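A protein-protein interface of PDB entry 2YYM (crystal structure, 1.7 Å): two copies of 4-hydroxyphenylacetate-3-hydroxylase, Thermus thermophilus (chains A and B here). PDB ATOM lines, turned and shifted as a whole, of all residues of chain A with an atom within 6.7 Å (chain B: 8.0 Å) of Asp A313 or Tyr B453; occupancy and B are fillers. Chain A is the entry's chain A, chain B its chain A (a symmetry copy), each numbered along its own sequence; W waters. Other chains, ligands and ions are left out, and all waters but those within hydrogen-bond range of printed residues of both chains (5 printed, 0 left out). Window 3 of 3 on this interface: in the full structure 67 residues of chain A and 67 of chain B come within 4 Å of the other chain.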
ATOM      1  N   ALA A 304       1.360 -10.468  -9.922  1.00  0.00           N
ATOM      2  CA  ALA A 304       1.264  -9.026  -9.728  1.00  0.00           C
ATOM      3  C   ALA A 304       0.600  -8.706  -8.392  1.00  0.00           C
ATOM      4  O   ALA A 304       1.078  -7.856  -7.644  1.00  0.00           O
ATOM      5  CB  ALA A 304       0.474  -8.391 -10.875  1.00  0.00           C
ATOM      6  N   MET A 306       0.296 -10.712  -5.702  1.00  0.00           N
ATOM      7  CA  MET A 306       1.091 -11.155  -4.564  1.00  0.00           C
ATOM      8  C   MET A 306       2.153 -10.111  -4.255  1.00  0.00           C
ATOM      9  O   MET A 306       2.299  -9.676  -3.116  1.00  0.00           O
ATOM     10  CB  MET A 306       1.785 -12.486  -4.855  1.00  0.00           C
ATOM     11  CG  MET A 306       0.942 -13.703  -4.565  1.00  0.00           C
ATOM     12  SD  MET A 306       1.965 -15.188  -4.553  1.00  0.00           S
ATOM     13  CE  MET A 306       2.178 -15.383  -6.270  1.00  0.00           C
ATOM     14  N   ALA A 307       2.892  -9.714  -5.286  1.00  0.00           N
ATOM     15  CA  ALA A 307       3.962  -8.735  -5.124  1.00  0.00           C
ATOM     16  C   ALA A 307       3.449  -7.420  -4.549  1.00  0.00           C
ATOM     17  O   ALA A 307       4.050  -6.849  -3.643  1.00  0.00           O
ATOM     18  CB  ALA A 307       4.648  -8.493  -6.462  1.00  0.00           C
ATOM     19  N   GLU A 308       2.335  -6.940  -5.082  1.00  0.00           N
ATOM     20  CA  GLU A 308       1.753  -5.692  -4.609  1.00  0.00           C
ATOM     21  C   GLU A 308       1.238  -5.889  -3.180  1.00  0.00           C
ATOM     22  O   GLU A 308       1.430  -5.037  -2.309  1.00  0.00           O
ATOM     23  CB  GLU A 308       0.607  -5.297  -5.537  1.00  0.00           C
ATOM     24  CG  GLU A 308      -0.018  -3.945  -5.269  1.00  0.00           C
ATOM     25  CD  GLU A 308      -1.097  -3.617  -6.286  1.00  0.00           C
ATOM     26  OE1 GLU A 308      -2.144  -4.293  -6.278  1.00  0.00           O
ATOM     27  OE2 GLU A 308      -0.891  -2.690  -7.098  1.00  0.00           O
ATOM     28  N   GLY A 309       0.606  -7.034  -2.950  1.00  0.00           N
ATOM     29  CA  GLY A 309       0.042  -7.341  -1.646  1.00  0.00           C
ATOM     30  C   GLY A 309       0.981  -7.324  -0.455  1.00  0.00           C
ATOM     31  O   GLY A 309       0.580  -6.919   0.642  1.00  0.00           O
ATOM     32  N   ILE A 310       2.219  -7.769  -0.647  1.00  0.00           N
ATOM     33  CA  ILE A 310       3.185  -7.791   0.446  1.00  0.00           C
ATOM     34  C   ILE A 310       4.265  -6.731   0.288  1.00  0.00           C
ATOM     35  O   ILE A 310       5.264  -6.749   1.003  1.00  0.00           O
ATOM     36  CB  ILE A 310       3.875  -9.172   0.579  1.00  0.00           C
ATOM     37  CG1 ILE A 310       4.606  -9.529  -0.719  1.00  0.00           C
ATOM     38  CG2 ILE A 310       2.847 -10.232   0.930  1.00  0.00           C
ATOM     39  CD1 ILE A 310       5.467 -10.784  -0.606  1.00  0.00           C
ATOM     40  N   GLY A 311       4.066  -5.816  -0.657  1.00  0.00           N
ATOM     41  CA  GLY A 311       5.030  -4.751  -0.868  1.00  0.00           C
ATOM     42  C   GLY A 311       6.351  -5.173  -1.484  1.00  0.00           C
ATOM     43  O   GLY A 311       7.347  -4.456  -1.378  1.00  0.00           O
ATOM     44  N   ALA A 312       6.378  -6.329  -2.133  1.00  0.00           N
ATOM     45  CA  ALA A 312       7.611  -6.796  -2.749  1.00  0.00           C
ATOM     46  C   ALA A 312       7.806  -6.204  -4.142  1.00  0.00           C
ATOM     47  O   ALA A 312       8.884  -6.323  -4.725  1.00  0.00           O
ATOM     48  CB  ALA A 312       7.615  -8.314  -2.825  1.00  0.00           C
ATOM     49  N   ASP A 313       6.767  -5.557  -4.665  1.00  0.00           N
ATOM     50  CA  ASP A 313       6.835  -4.966  -5.999  1.00  0.00           C
ATOM     51  C   ASP A 313       7.800  -3.783  -6.088  1.00  0.00           C
ATOM     52  O   ASP A 313       8.123  -3.318  -7.185  1.00  0.00           O
ATOM     53  CB  ASP A 313       5.431  -4.538  -6.452  1.00  0.00           C
ATOM     54  CG  ASP A 313       4.818  -3.490  -5.540  1.00  0.00           C
ATOM     55  OD1 ASP A 313       4.876  -3.662  -4.305  1.00  0.00           O
ATOM     56  OD2 ASP A 313       4.267  -2.496  -6.054  1.00  0.00           O
ATOM     57  N   VAL A 314       8.271  -3.291  -4.944  1.00  0.00           N
ATOM     58  CA  VAL A 314       9.206  -2.170  -4.962  1.00  0.00           C
ATOM     59  C   VAL A 314      10.624  -2.615  -5.306  1.00  0.00           C
ATOM     60  O   VAL A 314      11.484  -1.787  -5.607  1.00  0.00           O
ATOM     61  CB  VAL A 314       9.235  -1.424  -3.604  1.00  0.00           C
ATOM     62  CG1 VAL A 314       7.848  -0.871  -3.293  1.00  0.00           C
ATOM     63  CG2 VAL A 314       9.709  -2.352  -2.495  1.00  0.00           C
ATOM     64  N   TYR A 315      10.862  -3.924  -5.272  1.00  0.00           N
ATOM     65  CA  TYR A 315      12.182  -4.462  -5.573  1.00  0.00           C
ATOM     66  C   TYR A 315      12.363  -4.783  -7.050  1.00  0.00           C
ATOM     67  O   TYR A 315      11.541  -5.464  -7.656  1.00  0.00           O
ATOM     68  CB  TYR A 315      12.443  -5.698  -4.711  1.00  0.00           C
ATOM     69  CG  TYR A 315      12.448  -5.340  -3.247  1.00  0.00           C
ATOM     70  CD1 TYR A 315      13.451  -4.529  -2.722  1.00  0.00           C
ATOM     71  CD2 TYR A 315      11.397  -5.716  -2.411  1.00  0.00           C
ATOM     72  CE1 TYR A 315      13.408  -4.088  -1.405  1.00  0.00           C
ATOM     73  CE2 TYR A 315      11.342  -5.280  -1.085  1.00  0.00           C
ATOM     74  CZ  TYR A 315      12.351  -4.464  -0.593  1.00  0.00           C
ATOM     75  OH  TYR A 315      12.301  -4.002   0.703  1.00  0.00           O
ATOM     76  N   GLY A 316      13.457  -4.279  -7.612  1.00  0.00           N
ATOM     77  CA  GLY A 316      13.744  -4.489  -9.015  1.00  0.00           C
ATOM     78  C   GLY A 316      13.642  -5.917  -9.514  1.00  0.00           C
ATOM     79  O   GLY A 316      12.997  -6.171 -10.533  1.00  0.00           O
ATOM     80  N   VAL A 318      11.954  -8.338  -8.397  1.00  0.00           N
ATOM     81  CA  VAL A 318      10.577  -8.821  -8.369  1.00  0.00           C
ATOM     82  C   VAL A 318       9.866  -8.277  -9.610  1.00  0.00           C
ATOM     83  O   VAL A 318       9.095  -8.981 -10.262  1.00  0.00           O
ATOM     84  CB  VAL A 318       9.843  -8.358  -7.083  1.00  0.00           C
ATOM     85  CG1 VAL A 318       8.367  -8.716  -7.157  1.00  0.00           C
ATOM     86  CG2 VAL A 318      10.481  -9.023  -5.866  1.00  0.00           C
ATOM     87  N   GLN A 319      10.136  -7.017  -9.938  1.00  0.00           N
ATOM     88  CA  GLN A 319       9.541  -6.402 -11.115  1.00  0.00           C
ATOM     89  C   GLN A 319       9.999  -7.161 -12.359  1.00  0.00           C
ATOM     90  O   GLN A 319       9.208  -7.421 -13.269  1.00  0.00           O
ATOM     91  CB  GLN A 319       9.962  -4.933 -11.211  1.00  0.00           C
ATOM     92  CG  GLN A 319       9.477  -4.088 -10.035  1.00  0.00           C
ATOM     93  CD  GLN A 319       9.971  -2.658 -10.102  1.00  0.00           C
ATOM     94  OE1 GLN A 319      10.692  -2.281 -11.026  1.00  0.00           O
ATOM     95  NE2 GLN A 319       9.583  -1.849  -9.118  1.00  0.00           N
ATOM     96  N   GLU A 320      11.278  -7.523 -12.388  1.00  0.00           N
ATOM     97  CA  GLU A 320      11.832  -8.263 -13.513  1.00  0.00           C
ATOM     98  C   GLU A 320      11.150  -9.619 -13.692  1.00  0.00           C
ATOM     99  O   GLU A 320      10.844 -10.024 -14.814  1.00  0.00           O
ATOM    100  CB  GLU A 320      13.333  -8.454 -13.318  1.00  0.00           C
ATOM    101  CG  GLU A 320      14.123  -7.152 -13.415  1.00  0.00           C
ATOM    102  CD  GLU A 320      15.529  -7.296 -12.875  1.00  0.00           C
ATOM    103  OE1 GLU A 320      16.242  -8.221 -13.321  1.00  0.00           O
ATOM    104  OE2 GLU A 320      15.917  -6.484 -12.006  1.00  0.00           O
ATOM    105  N   ILE A 322       8.126 -10.458 -12.850  1.00  0.00           N
ATOM    106  CA  ILE A 322       6.784 -10.253 -13.370  1.00  0.00           C
ATOM    107  C   ILE A 322       6.872  -9.906 -14.860  1.00  0.00           C
ATOM    108  O   ILE A 322       6.079 -10.397 -15.660  1.00  0.00           O
ATOM    109  CB  ILE A 322       6.054  -9.147 -12.580  1.00  0.00           C
ATOM    110  CG1 ILE A 322       5.780  -9.653 -11.155  1.00  0.00           C
ATOM    111  CG2 ILE A 322       4.755  -8.771 -13.279  1.00  0.00           C
ATOM    112  CD1 ILE A 322       5.253  -8.594 -10.197  1.00  0.00           C
ATOM    113  N   ALA A 323       7.856  -9.089 -15.230  1.00  0.00           N
ATOM    114  CA  ALA A 323       8.038  -8.720 -16.633  1.00  0.00           C
ATOM    115  C   ALA A 323       8.364  -9.968 -17.458  1.00  0.00           C
ATOM    116  O   ALA A 323       8.022 -10.055 -18.639  1.00  0.00           O
ATOM    117  CB  ALA A 323       9.169  -7.689 -16.770  1.00  0.00           C
ATOM    118  N   ILE A 326       5.304 -11.475 -18.461  1.00  0.00           N
ATOM    119  CA  ILE A 326       4.693 -10.654 -19.502  1.00  0.00           C
ATOM    120  C   ILE A 326       5.294 -11.007 -20.862  1.00  0.00           C
ATOM    121  O   ILE A 326       4.579 -11.100 -21.863  1.00  0.00           O
ATOM    122  CB  ILE A 326       4.895  -9.146 -19.215  1.00  0.00           C
ATOM    123  CG1 ILE A 326       4.084  -8.749 -17.975  1.00  0.00           C
ATOM    124  CG2 ILE A 326       4.462  -8.314 -20.423  1.00  0.00           C
ATOM    125  CD1 ILE A 326       4.391  -7.351 -17.435  1.00  0.00           C
ATOM    126  N   ALA A 408       0.259  -5.111   2.583  1.00  0.00           N
ATOM    127  CA  ALA A 408       0.447  -3.679   2.406  1.00  0.00           C
ATOM    128  C   ALA A 408      -0.857  -3.167   1.807  1.00  0.00           C
ATOM    129  O   ALA A 408      -1.154  -3.421   0.634  1.00  0.00           O
ATOM    130  CB  ALA A 408       1.611  -3.412   1.455  1.00  0.00           C
ATOM    131  N   ASP B 359       7.961  -5.661 -27.632  1.00  0.00           N
ATOM    132  CA  ASP B 359       8.612  -5.668 -26.322  1.00  0.00           C
ATOM    133  C   ASP B 359       8.920  -7.126 -26.002  1.00  0.00           C
ATOM    134  O   ASP B 359       9.929  -7.440 -25.375  1.00  0.00           O
ATOM    135  CB  ASP B 359       7.699  -5.079 -25.238  1.00  0.00           C
ATOM    136  CG  ASP B 359       7.872  -3.576 -25.075  1.00  0.00           C
ATOM    137  OD1 ASP B 359       8.796  -3.009 -25.693  1.00  0.00           O
ATOM    138  OD2 ASP B 359       7.087  -2.962 -24.320  1.00  0.00           O
ATOM    139  N   ASN B 363      12.914  -8.337 -25.744  1.00  0.00           N
ATOM    140  CA  ASN B 363      13.283  -8.729 -24.392  1.00  0.00           C
ATOM    141  C   ASN B 363      13.508 -10.232 -24.308  1.00  0.00           C
ATOM    142  O   ASN B 363      14.112 -10.724 -23.354  1.00  0.00           O
ATOM    143  CB  ASN B 363      12.218  -8.282 -23.392  1.00  0.00           C
ATOM    144  CG  ASN B 363      12.380  -6.833 -23.005  1.00  0.00           C
ATOM    145  OD1 ASN B 363      13.397  -6.455 -22.425  1.00  0.00           O
ATOM    146  ND2 ASN B 363      11.392  -6.008 -23.336  1.00  0.00           N
ATOM    147  N   ARG B 447      17.215  -3.273 -16.574  1.00  0.00           N
ATOM    148  CA  ARG B 447      16.349  -2.112 -16.616  1.00  0.00           C
ATOM    149  C   ARG B 447      15.286  -2.179 -17.710  1.00  0.00           C
ATOM    150  O   ARG B 447      14.257  -1.512 -17.613  1.00  0.00           O
ATOM    151  CB  ARG B 447      17.199  -0.843 -16.714  1.00  0.00           C
ATOM    152  CG  ARG B 447      17.790  -0.472 -15.349  1.00  0.00           C
ATOM    153  CD  ARG B 447      18.916   0.530 -15.441  1.00  0.00           C
ATOM    154  NE  ARG B 447      20.123  -0.096 -15.964  1.00  0.00           N
ATOM    155  CZ  ARG B 447      21.228   0.570 -16.272  1.00  0.00           C
ATOM    156  NH1 ARG B 447      21.274   1.887 -16.103  1.00  0.00           N
ATOM    157  NH2 ARG B 447      22.279  -0.078 -16.757  1.00  0.00           N
ATOM    158  N   MET B 448      15.522  -2.980 -18.745  1.00  0.00           N
ATOM    159  CA  MET B 448      14.524  -3.117 -19.796  1.00  0.00           C
ATOM    160  C   MET B 448      13.341  -3.865 -19.191  1.00  0.00           C
ATOM    161  O   MET B 448      12.187  -3.531 -19.450  1.00  0.00           O
ATOM    162  CB  MET B 448      15.078  -3.905 -20.990  1.00  0.00           C
ATOM    163  CG  MET B 448      16.006  -3.090 -21.887  1.00  0.00           C
ATOM    164  SD  MET B 448      16.677  -4.069 -23.243  1.00  0.00           S
ATOM    165  CE  MET B 448      15.244  -4.236 -24.303  1.00  0.00           C
ATOM    166  N   TYR B 449      13.635  -4.874 -18.374  1.00  0.00           N
ATOM    167  CA  TYR B 449      12.571  -5.655 -17.747  1.00  0.00           C
ATOM    168  C   TYR B 449      11.831  -4.836 -16.698  1.00  0.00           C
ATOM    169  O   TYR B 449      10.613  -4.969 -16.538  1.00  0.00           O
ATOM    170  CB  TYR B 449      13.137  -6.938 -17.133  1.00  0.00           C
ATOM    171  CG  TYR B 449      13.167  -8.090 -18.117  1.00  0.00           C
ATOM    172  CD1 TYR B 449      13.870  -7.990 -19.316  1.00  0.00           C
ATOM    173  CD2 TYR B 449      12.456  -9.263 -17.868  1.00  0.00           C
ATOM    174  CE1 TYR B 449      13.860  -9.030 -20.245  1.00  0.00           C
ATOM    175  CE2 TYR B 449      12.437 -10.308 -18.789  1.00  0.00           C
ATOM    176  CZ  TYR B 449      13.138 -10.187 -19.974  1.00  0.00           C
ATOM    177  OH  TYR B 449      13.108 -11.221 -20.890  1.00  0.00           O
ATOM    178  N   GLN B 450      12.561  -3.995 -15.972  1.00  0.00           N
ATOM    179  CA  GLN B 450      11.922  -3.145 -14.974  1.00  0.00           C
ATOM    180  C   GLN B 450      11.023  -2.138 -15.692  1.00  0.00           C
ATOM    181  O   GLN B 450       9.935  -1.814 -15.215  1.00  0.00           O
ATOM    182  CB  GLN B 450      12.977  -2.424 -14.131  1.00  0.00           C
ATOM    183  CG  GLN B 450      13.615  -3.320 -13.087  1.00  0.00           C
ATOM    184  CD  GLN B 450      14.833  -2.697 -12.429  1.00  0.00           C
ATOM    185  OE1 GLN B 450      14.953  -1.477 -12.351  1.00  0.00           O
ATOM    186  NE2 GLN B 450      15.733  -3.538 -11.934  1.00  0.00           N
ATOM    187  N   THR B 451      11.475  -1.654 -16.849  1.00  0.00           N
ATOM    188  CA  THR B 451      10.691  -0.703 -17.631  1.00  0.00           C
ATOM    189  C   THR B 451       9.407  -1.366 -18.132  1.00  0.00           C
ATOM    190  O   THR B 451       8.330  -0.781 -18.053  1.00  0.00           O
ATOM    191  CB  THR B 451      11.487  -0.172 -18.855  1.00  0.00           C
ATOM    192  OG1 THR B 451      12.543   0.687 -18.406  1.00  0.00           O
ATOM    193  CG2 THR B 451      10.572   0.614 -19.790  1.00  0.00           C
ATOM    194  N   LEU B 452       9.529  -2.587 -18.644  1.00  0.00           N
ATOM    195  CA  LEU B 452       8.375  -3.317 -19.157  1.00  0.00           C
ATOM    196  C   LEU B 452       7.353  -3.518 -18.043  1.00  0.00           C
ATOM    197  O   LEU B 452       6.150  -3.363 -18.250  1.00  0.00           O
ATOM    198  CB  LEU B 452       8.812  -4.673 -19.722  1.00  0.00           C
ATOM    199  CG  LEU B 452       7.701  -5.621 -20.194  1.00  0.00           C
ATOM    200  CD1 LEU B 452       6.833  -4.933 -21.241  1.00  0.00           C
ATOM    201  CD2 LEU B 452       8.328  -6.896 -20.767  1.00  0.00           C
ATOM    202  N   TYR B 453       7.839  -3.860 -16.858  1.00  0.00           N
ATOM    203  CA  TYR B 453       6.947  -4.061 -15.724  1.00  0.00           C
ATOM    204  C   TYR B 453       6.130  -2.805 -15.435  1.00  0.00           C
ATOM    205  O   TYR B 453       4.911  -2.862 -15.260  1.00  0.00           O
ATOM    206  CB  TYR B 453       7.743  -4.413 -14.467  1.00  0.00           C
ATOM    207  CG  TYR B 453       6.901  -4.325 -13.213  1.00  0.00           C
ATOM    208  CD1 TYR B 453       6.013  -5.344 -12.874  1.00  0.00           C
ATOM    209  CD2 TYR B 453       6.944  -3.190 -12.404  1.00  0.00           C
ATOM    210  CE1 TYR B 453       5.180  -5.231 -11.753  1.00  0.00           C
ATOM    211  CE2 TYR B 453       6.116  -3.066 -11.286  1.00  0.00           C
ATOM    212  CZ  TYR B 453       5.239  -4.089 -10.969  1.00  0.00           C
ATOM    213  OH  TYR B 453       4.417  -3.962  -9.870  1.00  0.00           O
ATOM    214  N   ASN B 454       6.812  -1.670 -15.379  1.00  0.00           N
ATOM    215  CA  ASN B 454       6.154  -0.413 -15.067  1.00  0.00           C
ATOM    216  C   ASN B 454       5.195   0.133 -16.116  1.00  0.00           C
ATOM    217  O   ASN B 454       4.165   0.703 -15.765  1.00  0.00           O
ATOM    218  CB  ASN B 454       7.205   0.645 -14.715  1.00  0.00           C
ATOM    219  CG  ASN B 454       7.886   0.362 -13.382  1.00  0.00           C
ATOM    220  OD1 ASN B 454       9.048  -0.045 -13.332  1.00  0.00           O
ATOM    221  ND2 ASN B 454       7.153   0.563 -12.295  1.00  0.00           N
ATOM    222  N   VAL B 455       5.502  -0.051 -17.395  1.00  0.00           N
ATOM    223  CA  VAL B 455       4.631   0.482 -18.435  1.00  0.00           C
ATOM    224  C   VAL B 455       3.491  -0.430 -18.881  1.00  0.00           C
ATOM    225  O   VAL B 455       2.487   0.051 -19.409  1.00  0.00           O
ATOM    226  CB  VAL B 455       5.441   0.892 -19.692  1.00  0.00           C
ATOM    227  CG1 VAL B 455       6.554   1.852 -19.299  1.00  0.00           C
ATOM    228  CG2 VAL B 455       6.008  -0.339 -20.384  1.00  0.00           C
ATOM    229  N   TYR B 456       3.629  -1.732 -18.661  1.00  0.00           N
ATOM    230  CA  TYR B 456       2.600  -2.683 -19.079  1.00  0.00           C
ATOM    231  C   TYR B 456       1.320  -2.558 -18.254  1.00  0.00           C
ATOM    232  O   TYR B 456       1.376  -2.361 -17.044  1.00  0.00           O
ATOM    233  CB  TYR B 456       3.135  -4.112 -18.960  1.00  0.00           C
ATOM    234  CG  TYR B 456       2.412  -5.126 -19.821  1.00  0.00           C
ATOM    235  CD1 TYR B 456       2.641  -5.190 -21.195  1.00  0.00           C
ATOM    236  CD2 TYR B 456       1.527  -6.047 -19.255  1.00  0.00           C
ATOM    237  CE1 TYR B 456       2.016  -6.152 -21.991  1.00  0.00           C
ATOM    238  CE2 TYR B 456       0.894  -7.015 -20.041  1.00  0.00           C
ATOM    239  CZ  TYR B 456       1.149  -7.065 -21.407  1.00  0.00           C
ATOM    240  OH  TYR B 456       0.571  -8.047 -22.179  1.00  0.00           O
ATOM    241  N   ASN B 457       0.170  -2.672 -18.910  1.00  0.00           N
ATOM    242  CA  ASN B 457      -1.108  -2.600 -18.207  1.00  0.00           C
ATOM    243  C   ASN B 457      -1.418  -3.980 -17.632  1.00  0.00           C
ATOM    244  O   ASN B 457      -1.843  -4.883 -18.350  1.00  0.00           O
ATOM    245  CB  ASN B 457      -2.227  -2.166 -19.161  1.00  0.00           C
ATOM    246  CG  ASN B 457      -3.586  -2.140 -18.484  1.00  0.00           C
ATOM    247  OD1 ASN B 457      -3.678  -2.113 -17.252  1.00  0.00           O
ATOM    248  ND2 ASN B 457      -4.646  -2.135 -19.285  1.00  0.00           N
ATOM    249  N   LYS B 458      -1.200  -4.127 -16.330  1.00  0.00           N
ATOM    250  CA  LYS B 458      -1.419  -5.393 -15.637  1.00  0.00           C
ATOM    251  C   LYS B 458      -2.796  -5.493 -14.994  1.00  0.00           C
ATOM    252  O   LYS B 458      -3.180  -6.549 -14.493  1.00  0.00           O
ATOM    253  CB  LYS B 458      -0.348  -5.567 -14.558  1.00  0.00           C
ATOM    254  CG  LYS B 458       1.080  -5.508 -15.094  1.00  0.00           C
ATOM    255  CD  LYS B 458       2.105  -5.318 -13.982  1.00  0.00           C
ATOM    256  CE  LYS B 458       2.020  -3.928 -13.353  1.00  0.00           C
ATOM    257  NZ  LYS B 458       2.349  -2.836 -14.319  1.00  0.00           N
ATOM    258  N   GLU B 459      -3.547  -4.398 -15.023  1.00  0.00           N
ATOM    259  CA  GLU B 459      -4.860  -4.371 -14.391  1.00  0.00           C
ATOM    260  C   GLU B 459      -5.888  -5.424 -14.806  1.00  0.00           C
ATOM    261  O   GLU B 459      -6.549  -6.008 -13.949  1.00  0.00           O
ATOM    262  CB  GLU B 459      -5.461  -2.974 -14.522  1.00  0.00           C
ATOM    263  CG  GLU B 459      -4.612  -1.912 -13.847  1.00  0.00           C
ATOM    264  CD  GLU B 459      -4.196  -2.309 -12.439  1.00  0.00           C
ATOM    265  OE1 GLU B 459      -5.088  -2.593 -11.611  1.00  0.00           O
ATOM    266  OE2 GLU B 459      -2.976  -2.336 -12.160  1.00  0.00           O
ATOM    267  N   LYS B 462      -5.168  -8.684 -13.044  1.00  0.00           N
ATOM    268  CA  LYS B 462      -5.383  -8.576 -11.610  1.00  0.00           C
ATOM    269  C   LYS B 462      -6.889  -8.581 -11.345  1.00  0.00           C
ATOM    270  O   LYS B 462      -7.357  -9.215 -10.396  1.00  0.00           O
ATOM    271  CB  LYS B 462      -4.738  -7.291 -11.084  1.00  0.00           C
ATOM    272  CG  LYS B 462      -3.210  -7.325 -11.145  1.00  0.00           C
ATOM    273  CD  LYS B 462      -2.585  -5.931 -11.096  1.00  0.00           C
ATOM    274  CE  LYS B 462      -2.788  -5.244  -9.756  1.00  0.00           C
ATOM    275  NZ  LYS B 462      -2.171  -3.879  -9.767  1.00  0.00           N
HETATM  276  O   HOH W   1       8.659   1.239  -9.982  1.00  0.00           O
HETATM  277  O   HOH W   2      -4.279  -3.475  -7.590  1.00  0.00           O
HETATM  278  O   HOH W   3      12.332  -0.169 -10.796  1.00  0.00           O
HETATM  279  O   HOH W   4       2.555  -5.980  -8.956  1.00  0.00           O
HETATM  280  O   HOH W   5       4.265  -1.590  -8.499  1.00  0.00           O
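O of Ala A307 lies within hydrogen-bond range of N of Asp A313, 3.2 Å away. O of Asp A313 sits at hydrogen-bond distance from NE2 of Gln A319 (2.8 Å). The backbone carbonyl oxygen of Asn B363 lies within hydrogen-bond range of the side-chain hydroxyl of Tyr B449 (2.7 Å). The side-chain amide oxygen (OD1) of Asn B454 sits close to the backbone carbonyl oxygen (O) of Gln B450 (2.7 Å). The side-chain amino group of Lys B458 is in hydrogen-bond range of the backbone carbonyl oxygen of Tyr B453. The side-chain carboxylate (OE2) of Glu B459 lies within salt-bridge range of the side-chain amino group (NZ) of Lys B462 (3.0 Å).
Ala A304 touches Lys B462. CB of Asp A313 touches OH of Tyr B453, 3.6 Å away. NE2 of Gln B450 touches CA of Gly A316 (3.7 Å). Gln A319 touches Gln B450 (OE1 to CG, 3.7 Å). Gln A319 touches Tyr B453. OE1 of Gln A319 touches OD1 of Asn B454 (3.6 Å). CG2 of Ile A322 touches CD1 of Tyr B453 (3.7 Å). Ala A323 touches Tyr B449. Ala A323 touches Leu B452. Ile A326 touches Tyr B456.
Water W5 lies within hydrogen-bond range of OD2 of Asp A313 (2.6 Å) and OH of Tyr B453 (2.7 Å). Water W2 lies within hydrogen-bond range of the side-chain carboxylate (OE1) of Glu A308 (2.6 Å) and the side-chain amino group (NZ) of Lys B462 (3.1 Å). Water W3 lies within hydrogen-bond range of OE1 of Gln A319 and OE1 of Gln B450. Water W4 bridges the backbone carbonyl oxygen (O) of Ala A304 and the side-chain hydroxyl (OH) of Tyr B453. Water W1 bridges ND2 of Asn B454 (2.8 Å) and NE2 of Gln A319 (3.3 Å).
Of the 16 printed residues of chain B, 7 touch a printed residue of chain A. Hydrophobic or aromatic side chains of chain B within 4 Å of the printed part of chain A: Tyr B449, Leu B452, Tyr B453 and Tyr B456. Hydrophobic or aromatic side chains of chain A that line the printed part of chain B: Ala A304, Ile A322, Ala A323 and Ile A326. Among the printed residues, 13 pairs touch across the chains. Among the printed residues, Asp or Glu carboxylates within 4 Å of a Lys or Arg side-chain nitrogen of the other chain: Glu A308 with Lys B462.
No position is printed for both chains. Of the 13 pairs that touch across the chains among the printed residues, none has its exchanged pair printed and touching as well.
OE2 of Glu A308 is in salt-bridge range of NZ of Lys B462, 3.2 Å away. OE2 of Glu A320 is in hydrogen-bond range of NE2 of Gln B450, 3.0 Å away.
Of the printed residues of chain B, Ala A304 touches Lys B462 (3.8 Å). No residue of chain B comes within 4 Å of Ala A312. Of chain B, only Tyr B453 comes within 4 Å of Asp A313. Of the printed residues of chain B, Ile A322 touches Tyr B453 (3.7 Å). Of the printed residues of chain B, Ile A326 touches Tyr B456 (3.6 Å). Met B448 touches none of the printed residues of chain A. The nearest residue of chain B that does not touch Asp A313 is Asn B454 (6.5 Å). The nearest residue of chain A that does not touch Tyr B453 is Ala A323 (4.1 Å). The nearest printed residue of chain A that does not touch Asn B454 is Asp A313 (6.5 Å).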
